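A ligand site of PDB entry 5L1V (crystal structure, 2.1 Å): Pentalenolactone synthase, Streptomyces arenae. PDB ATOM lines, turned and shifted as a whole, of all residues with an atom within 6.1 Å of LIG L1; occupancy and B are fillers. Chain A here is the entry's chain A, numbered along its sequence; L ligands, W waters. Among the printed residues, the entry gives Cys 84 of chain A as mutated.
Water W3 lies within hydrogen-bond range of O of Asn 286 (2.8 Å) and O1 of LIG L1 (2.9 Å).
Water W2 lies within hydrogen-bond range of the guanidinium group of Arg 243, an oxygen (O3) of LIG L1, the backbone carbonyl oxygen of Thr 391 and the side-chain amide nitrogen of Asn 286.
Water W1 bridges an oxygen (O2) of LG2 L2 and an oxygen (O2) of LIG L1.
SD of Met 80 touches C8 of LIG L1 (3.8 Å).
Phe 235 touches LIG L1.
Thr 239 touches LIG L1 (CG2 to C9, 3.5 Å).
Leu 288 touches LIG L1.
CG1 of Ile 289 touches O5 of LIG L1, at 3.8 Å.
Pro 290 touches LIG L1 (CD to O2, 3.5 Å).
CG2 of Ile 390 touches O4 of LIG L1 (3.3 Å).
Thr 391 touches LIG L1.
Hydrophobic or aromatic side chains that line LIG L1: Met 80, Phe 235, Ile 289, Pro 290 and Ile 390.
NH1 of Arg 243 is in hydrogen-bond range of O of Thr 239 (3.1 Å).
The backbone NH (N) of Ile 390 lies within hydrogen-bond range of the backbone carbonyl oxygen (O) of Phe 174, 3.0 Å away.
The backbone carbonyl oxygen (O) of Met 80 sits at hydrogen-bond distance from the side-chain sulfur (SG) of Cys 84 (3.5 Å).
The guanidinium group of Arg 243 is in salt-bridge range of an oxygen (O1) of LIG L1 (2.9 Å).
NH1 of Arg 77 is in hydrogen-bond range of O2 of LIG L1 (2.9 Å).
The side-chain amide nitrogen of Asn 286 sits close to an oxygen (O3) of LIG L1 (3.3 Å).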
ATOM      1  N   ARG A  77     -29.293 -17.911   2.138  1.00  0.00           N
ATOM      2  CA  ARG A  77     -28.636 -17.476   3.370  1.00  0.00           C
ATOM      3  C   ARG A  77     -28.475 -18.619   4.357  1.00  0.00           C
ATOM      4  O   ARG A  77     -27.490 -18.669   5.100  1.00  0.00           O
ATOM      5  CB  ARG A  77     -29.433 -16.346   4.022  1.00  0.00           C
ATOM      6  CG  ARG A  77     -29.130 -14.976   3.491  1.00  0.00           C
ATOM      7  CD  ARG A  77     -27.729 -14.498   3.921  1.00  0.00           C
ATOM      8  NE  ARG A  77     -27.432 -13.195   3.330  1.00  0.00           N
ATOM      9  CZ  ARG A  77     -26.259 -12.582   3.380  1.00  0.00           C
ATOM     10  NH1 ARG A  77     -25.214 -13.145   4.008  1.00  0.00           N
ATOM     11  NH2 ARG A  77     -26.121 -11.399   2.800  1.00  0.00           N
ATOM     12  N   MET A  80     -25.475 -20.670   3.281  1.00  0.00           N
ATOM     13  CA  MET A  80     -24.271 -19.907   3.574  1.00  0.00           C
ATOM     14  C   MET A  80     -23.904 -19.996   5.053  1.00  0.00           C
ATOM     15  O   MET A  80     -22.747 -20.223   5.403  1.00  0.00           O
ATOM     16  CB  MET A  80     -24.449 -18.449   3.139  1.00  0.00           C
ATOM     17  CG  MET A  80     -23.224 -17.577   3.444  1.00  0.00           C
ATOM     18  SD  MET A  80     -23.189 -16.014   2.525  1.00  0.00           S
ATOM     19  CE  MET A  80     -22.765 -16.632   0.892  1.00  0.00           C
ATOM     20  N   CYS A  84     -20.718 -22.028   7.090  1.00  0.00           N
ATOM     21  CA  CYS A  84     -19.855 -21.288   8.015  1.00  0.00           C
ATOM     22  C   CYS A  84     -19.976 -21.797   9.450  1.00  0.00           C
ATOM     23  O   CYS A  84     -19.478 -21.135  10.366  1.00  0.00           O
ATOM     24  CB  CYS A  84     -20.191 -19.785   7.971  1.00  0.00           C
ATOM     25  SG  CYS A  84     -19.719 -18.894   6.428  1.00  0.00           S
ATOM     26  N   PHE A 174     -26.474 -19.362  -3.928  1.00  0.00           N
ATOM     27  CA  PHE A 174     -26.700 -18.103  -3.233  1.00  0.00           C
ATOM     28  C   PHE A 174     -27.710 -17.204  -3.953  1.00  0.00           C
ATOM     29  O   PHE A 174     -27.665 -15.978  -3.810  1.00  0.00           O
ATOM     30  CB  PHE A 174     -25.368 -17.391  -3.005  1.00  0.00           C
ATOM     31  CG  PHE A 174     -24.391 -18.226  -2.211  1.00  0.00           C
ATOM     32  CD1 PHE A 174     -24.847 -19.036  -1.179  1.00  0.00           C
ATOM     33  CD2 PHE A 174     -23.030 -18.225  -2.512  1.00  0.00           C
ATOM     34  CE1 PHE A 174     -23.961 -19.829  -0.444  1.00  0.00           C
ATOM     35  CE2 PHE A 174     -22.150 -19.002  -1.792  1.00  0.00           C
ATOM     36  CZ  PHE A 174     -22.608 -19.821  -0.762  1.00  0.00           C
ATOM     37  N   LEU A 234     -17.633 -23.240  -2.794  1.00  0.00           N
ATOM     38  CA  LEU A 234     -18.637 -22.183  -2.917  1.00  0.00           C
ATOM     39  C   LEU A 234     -18.154 -20.812  -2.458  1.00  0.00           C
ATOM     40  O   LEU A 234     -18.698 -19.789  -2.891  1.00  0.00           O
ATOM     41  CB  LEU A 234     -19.910 -22.577  -2.172  1.00  0.00           C
ATOM     42  CG  LEU A 234     -20.702 -23.763  -2.758  1.00  0.00           C
ATOM     43  CD1 LEU A 234     -21.601 -24.432  -1.706  1.00  0.00           C
ATOM     44  CD2 LEU A 234     -21.552 -23.322  -3.929  1.00  0.00           C
ATOM     45  N   PHE A 235     -17.106 -20.756  -1.619  1.00  0.00           N
ATOM     46  CA  PHE A 235     -16.493 -19.468  -1.262  1.00  0.00           C
ATOM     47  C   PHE A 235     -15.207 -19.194  -2.014  1.00  0.00           C
ATOM     48  O   PHE A 235     -14.724 -18.053  -2.007  1.00  0.00           O
ATOM     49  CB  PHE A 235     -16.199 -19.418   0.257  1.00  0.00           C
ATOM     50  CG  PHE A 235     -17.402 -19.668   1.146  1.00  0.00           C
ATOM     51  CD1 PHE A 235     -17.221 -20.117   2.446  1.00  0.00           C
ATOM     52  CD2 PHE A 235     -18.712 -19.433   0.691  1.00  0.00           C
ATOM     53  CE1 PHE A 235     -18.309 -20.366   3.296  1.00  0.00           C
ATOM     54  CE2 PHE A 235     -19.815 -19.670   1.552  1.00  0.00           C
ATOM     55  CZ  PHE A 235     -19.603 -20.140   2.854  1.00  0.00           C
ATOM     56  N   THR A 239     -16.278 -14.887  -5.389  1.00  0.00           N
ATOM     57  CA  THR A 239     -15.956 -13.527  -4.956  1.00  0.00           C
ATOM     58  C   THR A 239     -14.667 -13.030  -5.586  1.00  0.00           C
ATOM     59  O   THR A 239     -14.515 -11.818  -5.811  1.00  0.00           O
ATOM     60  CB  THR A 239     -15.862 -13.448  -3.418  1.00  0.00           C
ATOM     61  OG1 THR A 239     -14.930 -14.414  -2.923  1.00  0.00           O
ATOM     62  CG2 THR A 239     -17.227 -13.633  -2.757  1.00  0.00           C
ATOM     63  N   ARG A 243     -14.027  -9.618  -7.876  1.00  0.00           N
ATOM     64  CA  ARG A 243     -12.988  -8.609  -7.644  1.00  0.00           C
ATOM     65  C   ARG A 243     -12.145  -8.353  -8.894  1.00  0.00           C
ATOM     66  O   ARG A 243     -11.661  -7.235  -9.082  1.00  0.00           O
ATOM     67  CB  ARG A 243     -12.087  -9.034  -6.467  1.00  0.00           C
ATOM     68  CG  ARG A 243     -12.803  -9.006  -5.090  1.00  0.00           C
ATOM     69  CD  ARG A 243     -13.957  -7.980  -5.101  1.00  0.00           C
ATOM     70  NE  ARG A 243     -14.692  -7.863  -3.832  1.00  0.00           N
ATOM     71  CZ  ARG A 243     -15.680  -8.666  -3.457  1.00  0.00           C
ATOM     72  NH1 ARG A 243     -16.055  -9.681  -4.230  1.00  0.00           N
ATOM     73  NH2 ARG A 243     -16.320  -8.437  -2.302  1.00  0.00           N
ATOM     74  N   SER A 285     -24.920  -4.889  -1.264  1.00  0.00           N
ATOM     75  CA  SER A 285     -25.448  -5.694  -0.174  1.00  0.00           C
ATOM     76  C   SER A 285     -24.480  -6.791   0.251  1.00  0.00           C
ATOM     77  O   SER A 285     -24.617  -7.327   1.368  1.00  0.00           O
ATOM     78  CB  SER A 285     -26.791  -6.317  -0.560  1.00  0.00           C
ATOM     79  OG  SER A 285     -27.758  -5.302  -0.845  1.00  0.00           O
ATOM     80  N   ASN A 286     -23.526  -7.159  -0.598  1.00  0.00           N
ATOM     81  CA  ASN A 286     -22.528  -8.134  -0.218  1.00  0.00           C
ATOM     82  C   ASN A 286     -21.379  -7.525   0.574  1.00  0.00           C
ATOM     83  O   ASN A 286     -20.560  -8.251   1.133  1.00  0.00           O
ATOM     84  CB  ASN A 286     -21.953  -8.826  -1.459  1.00  0.00           C
ATOM     85  CG  ASN A 286     -21.283  -7.853  -2.405  1.00  0.00           C
ATOM     86  OD1 ASN A 286     -21.825  -6.779  -2.715  1.00  0.00           O
ATOM     87  ND2 ASN A 286     -20.098  -8.211  -2.864  1.00  0.00           N
ATOM     88  N   ALA A 287     -21.289  -6.198   0.620  1.00  0.00           N
ATOM     89  CA  ALA A 287     -20.302  -5.509   1.446  1.00  0.00           C
ATOM     90  C   ALA A 287     -20.840  -5.223   2.835  1.00  0.00           C
ATOM     91  O   ALA A 287     -20.445  -4.230   3.474  1.00  0.00           O
ATOM     92  CB  ALA A 287     -19.804  -4.245   0.751  1.00  0.00           C
ATOM     93  N   LEU A 288     -21.755  -6.054   3.318  1.00  0.00           N
ATOM     94  CA  LEU A 288     -22.250  -6.032   4.687  1.00  0.00           C
ATOM     95  C   LEU A 288     -21.967  -7.386   5.303  1.00  0.00           C
ATOM     96  O   LEU A 288     -22.308  -8.419   4.717  1.00  0.00           O
ATOM     97  CB  LEU A 288     -23.746  -5.739   4.722  1.00  0.00           C
ATOM     98  CG  LEU A 288     -24.252  -4.450   4.063  1.00  0.00           C
ATOM     99  CD1 LEU A 288     -25.766  -4.420   4.094  1.00  0.00           C
ATOM    100  CD2 LEU A 288     -23.682  -3.245   4.767  1.00  0.00           C
ATOM    101  N   ILE A 289     -21.338  -7.400   6.473  1.00  0.00           N
ATOM    102  CA  ILE A 289     -21.099  -8.619   7.232  1.00  0.00           C
ATOM    103  C   ILE A 289     -22.175  -8.720   8.310  1.00  0.00           C
ATOM    104  O   ILE A 289     -22.246  -7.830   9.173  1.00  0.00           O
ATOM    105  CB  ILE A 289     -19.696  -8.647   7.856  1.00  0.00           C
ATOM    106  CG1 ILE A 289     -18.626  -8.767   6.763  1.00  0.00           C
ATOM    107  CG2 ILE A 289     -19.584  -9.798   8.885  1.00  0.00           C
ATOM    108  CD1 ILE A 289     -17.187  -8.827   7.312  1.00  0.00           C
ATOM    109  N   PRO A 290     -23.039  -9.729   8.292  1.00  0.00           N
ATOM    110  CA  PRO A 290     -24.148  -9.774   9.243  1.00  0.00           C
ATOM    111  C   PRO A 290     -23.761 -10.484  10.535  1.00  0.00           C
ATOM    112  O   PRO A 290     -22.985 -11.438  10.556  1.00  0.00           O
ATOM    113  CB  PRO A 290     -25.218 -10.566   8.482  1.00  0.00           C
ATOM    114  CG  PRO A 290     -24.432 -11.506   7.620  1.00  0.00           C
ATOM    115  CD  PRO A 290     -23.106 -10.825   7.303  1.00  0.00           C
ATOM    116  N   ILE A 314     -18.552  -3.159   5.820  1.00  0.00           N
ATOM    117  CA  ILE A 314     -17.125  -3.135   5.487  1.00  0.00           C
ATOM    118  C   ILE A 314     -16.876  -2.276   4.252  1.00  0.00           C
ATOM    119  O   ILE A 314     -15.832  -1.616   4.145  1.00  0.00           O
ATOM    120  CB  ILE A 314     -16.590  -4.578   5.304  1.00  0.00           C
ATOM    121  CG1 ILE A 314     -17.391  -5.340   4.239  1.00  0.00           C
ATOM    122  CG2 ILE A 314     -16.604  -5.331   6.617  1.00  0.00           C
ATOM    123  CD1 ILE A 314     -16.818  -6.738   3.893  1.00  0.00           C
ATOM    124  N   ALA A 342     -12.023  -5.481   3.605  1.00  0.00           N
ATOM    125  CA  ALA A 342     -12.731  -6.245   2.568  1.00  0.00           C
ATOM    126  C   ALA A 342     -12.642  -7.759   2.752  1.00  0.00           C
ATOM    127  O   ALA A 342     -13.455  -8.483   2.148  1.00  0.00           O
ATOM    128  CB  ALA A 342     -12.201  -5.886   1.183  1.00  0.00           C
ATOM    129  N   ILE A 390     -26.304 -13.384  -3.300  1.00  0.00           N
ATOM    130  CA  ILE A 390     -25.602 -12.922  -2.100  1.00  0.00           C
ATOM    131  C   ILE A 390     -24.270 -12.301  -2.478  1.00  0.00           C
ATOM    132  O   ILE A 390     -23.865 -11.267  -1.920  1.00  0.00           O
ATOM    133  CB  ILE A 390     -25.407 -14.058  -1.091  1.00  0.00           C
ATOM    134  CG1 ILE A 390     -26.763 -14.590  -0.584  1.00  0.00           C
ATOM    135  CG2 ILE A 390     -24.587 -13.570   0.091  1.00  0.00           C
ATOM    136  CD1 ILE A 390     -26.645 -15.848   0.283  1.00  0.00           C
ATOM    137  N   THR A 391     -23.576 -12.897  -3.443  1.00  0.00           N
ATOM    138  CA  THR A 391     -22.265 -12.464  -3.899  1.00  0.00           C
ATOM    139  C   THR A 391     -22.332 -11.444  -5.046  1.00  0.00           C
ATOM    140  O   THR A 391     -21.277 -11.076  -5.589  1.00  0.00           O
ATOM    141  CB  THR A 391     -21.441 -13.689  -4.310  1.00  0.00           C
ATOM    142  OG1 THR A 391     -22.251 -14.545  -5.141  1.00  0.00           O
ATOM    143  CG2 THR A 391     -21.024 -14.490  -3.067  1.00  0.00           C
ATOM    144  N   GLY A 392     -23.531 -10.992  -5.429  1.00  0.00           N
ATOM    145  CA  GLY A 392     -23.652  -9.922  -6.428  1.00  0.00           C
ATOM    146  C   GLY A 392     -22.973 -10.256  -7.746  1.00  0.00           C
ATOM    147  O   GLY A 392     -23.161 -11.340  -8.304  1.00  0.00           O
HETATM  148  C1  LIG L   1     -17.474 -14.089   2.305  1.00  0.00           C
HETATM  149  C2  LIG L   1     -18.607 -15.107   2.204  1.00  0.00           C
HETATM  150  C3  LIG L   1     -18.341 -16.287   3.141  1.00  0.00           C
HETATM  151  C4  LIG L   1     -18.751 -15.640   0.764  1.00  0.00           C
HETATM  152  C5  LIG L   1     -17.926 -11.889   1.088  1.00  0.00           C
HETATM  153  C6  LIG L   1     -21.334 -11.749   0.816  1.00  0.00           C
HETATM  154  C7  LIG L   1     -19.817 -10.480   3.571  1.00  0.00           C
HETATM  155  C8  LIG L   1     -19.841 -14.327   2.736  1.00  0.00           C
HETATM  156  C9  LIG L   1     -19.010 -11.198  -0.915  1.00  0.00           C
HETATM  157  C10 LIG L   1     -21.774 -12.062   3.157  1.00  0.00           C
HETATM  158  C11 LIG L   1     -18.989 -11.899   0.252  1.00  0.00           C
HETATM  159  C12 LIG L   1     -18.141 -12.658   2.274  1.00  0.00           C
HETATM  160  C13 LIG L   1     -20.051 -12.642   0.799  1.00  0.00           C
HETATM  161  C14 LIG L   1     -20.376 -11.876   3.239  1.00  0.00           C
HETATM  162  C15 LIG L   1     -19.655 -12.863   2.259  1.00  0.00           C
HETATM  163  O1  LIG L   1     -18.062 -10.456  -1.262  1.00  0.00           O
HETATM  164  O2  LIG L   1     -22.451 -12.277   4.164  1.00  0.00           O
HETATM  165  O3  LIG L   1     -19.957 -11.292  -1.720  1.00  0.00           O
HETATM  166  O4  LIG L   1     -22.291 -12.073   1.880  1.00  0.00           O
HETATM  167  O5  LIG L   1     -19.784 -11.598   4.520  1.00  0.00           O
HETATM  168  C1  LG2 L   2     -14.669 -15.481   4.906  1.00  0.00           C
HETATM  169  C2  LG2 L   2     -14.120 -12.030   1.544  1.00  0.00           C
HETATM  170  C3  LG2 L   2     -11.789 -15.147  -1.349  1.00  0.00           C
HETATM  171  C4  LG2 L   2     -12.522 -18.691   1.873  1.00  0.00           C
HETATM  172  C5  LG2 L   2     -14.689 -14.237   4.305  1.00  0.00           C
HETATM  173  C6  LG2 L   2     -15.168 -12.975   4.857  1.00  0.00           C
HETATM  174  C7  LG2 L   2     -15.005 -12.039   3.900  1.00  0.00           C
HETATM  175  C8  LG2 L   2     -14.417 -12.658   2.729  1.00  0.00           C
HETATM  176  C9  LG2 L   2     -15.375 -10.531   3.989  1.00  0.00           C
HETATM  177  C10 LG2 L   2     -15.732 -12.703   6.287  1.00  0.00           C
HETATM  178  C11 LG2 L   2     -17.121 -13.308   6.546  1.00  0.00           C
HETATM  179  C12 LG2 L   2     -17.587 -12.982   7.953  1.00  0.00           C
HETATM  180  O1  LG2 L   2     -16.838 -12.240   8.673  1.00  0.00           O
HETATM  181  O2  LG2 L   2     -18.693 -13.459   8.359  1.00  0.00           O
HETATM  182  C13 LG2 L   2     -13.449 -12.551   0.445  1.00  0.00           C
HETATM  183  C14 LG2 L   2     -13.059 -11.837  -0.760  1.00  0.00           C
HETATM  184  C15 LG2 L   2     -12.424 -12.721  -1.557  1.00  0.00           C
HETATM  185  C16 LG2 L   2     -12.365 -14.000  -0.870  1.00  0.00           C
HETATM  186  C17 LG2 L   2     -13.366 -10.349  -1.056  1.00  0.00           C
HETATM  187  C18 LG2 L   2     -11.788 -12.517  -2.957  1.00  0.00           C
HETATM  188  C19 LG2 L   2     -11.128 -11.392  -3.267  1.00  0.00           C
HETATM  189  C20 LG2 L   2     -11.744 -16.372  -0.728  1.00  0.00           C
HETATM  190  C21 LG2 L   2     -11.022 -17.529  -1.206  1.00  0.00           C
HETATM  191  C22 LG2 L   2     -11.225 -18.522  -0.312  1.00  0.00           C
HETATM  192  C23 LG2 L   2     -12.070 -18.008   0.757  1.00  0.00           C
HETATM  193  C24 LG2 L   2     -10.184 -17.520  -2.529  1.00  0.00           C
HETATM  194  C25 LG2 L   2     -10.727 -19.993  -0.315  1.00  0.00           C
HETATM  195  C26 LG2 L   2     -10.169 -20.591  -1.371  1.00  0.00           C
HETATM  196  C27 LG2 L   2     -13.218 -18.155   2.942  1.00  0.00           C
HETATM  197  C28 LG2 L   2     -13.817 -18.880   4.048  1.00  0.00           C
HETATM  198  C29 LG2 L   2     -14.405 -17.995   4.871  1.00  0.00           C
HETATM  199  C30 LG2 L   2     -14.215 -16.664   4.327  1.00  0.00           C
HETATM  200  C31 LG2 L   2     -13.763 -20.406   4.232  1.00  0.00           C
HETATM  201  C32 LG2 L   2     -15.159 -18.302   6.178  1.00  0.00           C
HETATM  202  C33 LG2 L   2     -14.320 -17.863   7.366  1.00  0.00           C
HETATM  203  C34 LG2 L   2     -15.010 -18.124   8.674  1.00  0.00           C
HETATM  204  O3  LG2 L   2     -14.259 -18.408   9.648  1.00  0.00           O
HETATM  205  O4  LG2 L   2     -16.276 -18.039   8.757  1.00  0.00           O
HETATM  206  N1  LG2 L   2     -14.225 -14.007   3.027  1.00  0.00           N
HETATM  207  N2  LG2 L   2     -12.999 -13.853   0.344  1.00  0.00           N
HETATM  208  N3  LG2 L   2     -12.365 -16.696   0.467  1.00  0.00           N
HETATM  209  N4  LG2 L   2     -13.494 -16.802   3.150  1.00  0.00           N
HETATM  210 FE1  LG2 L   2     -13.042 -15.270   1.836  1.00  0.00          FE
HETATM  211  O   HOH W   1     -21.129 -13.357   6.640  1.00  0.00           O
HETATM  212  O   HOH W   2     -18.578 -10.775  -4.315  1.00  0.00           O
HETATM  213  O   HOH W   3     -17.833  -8.600   0.983  1.00  0.00           O
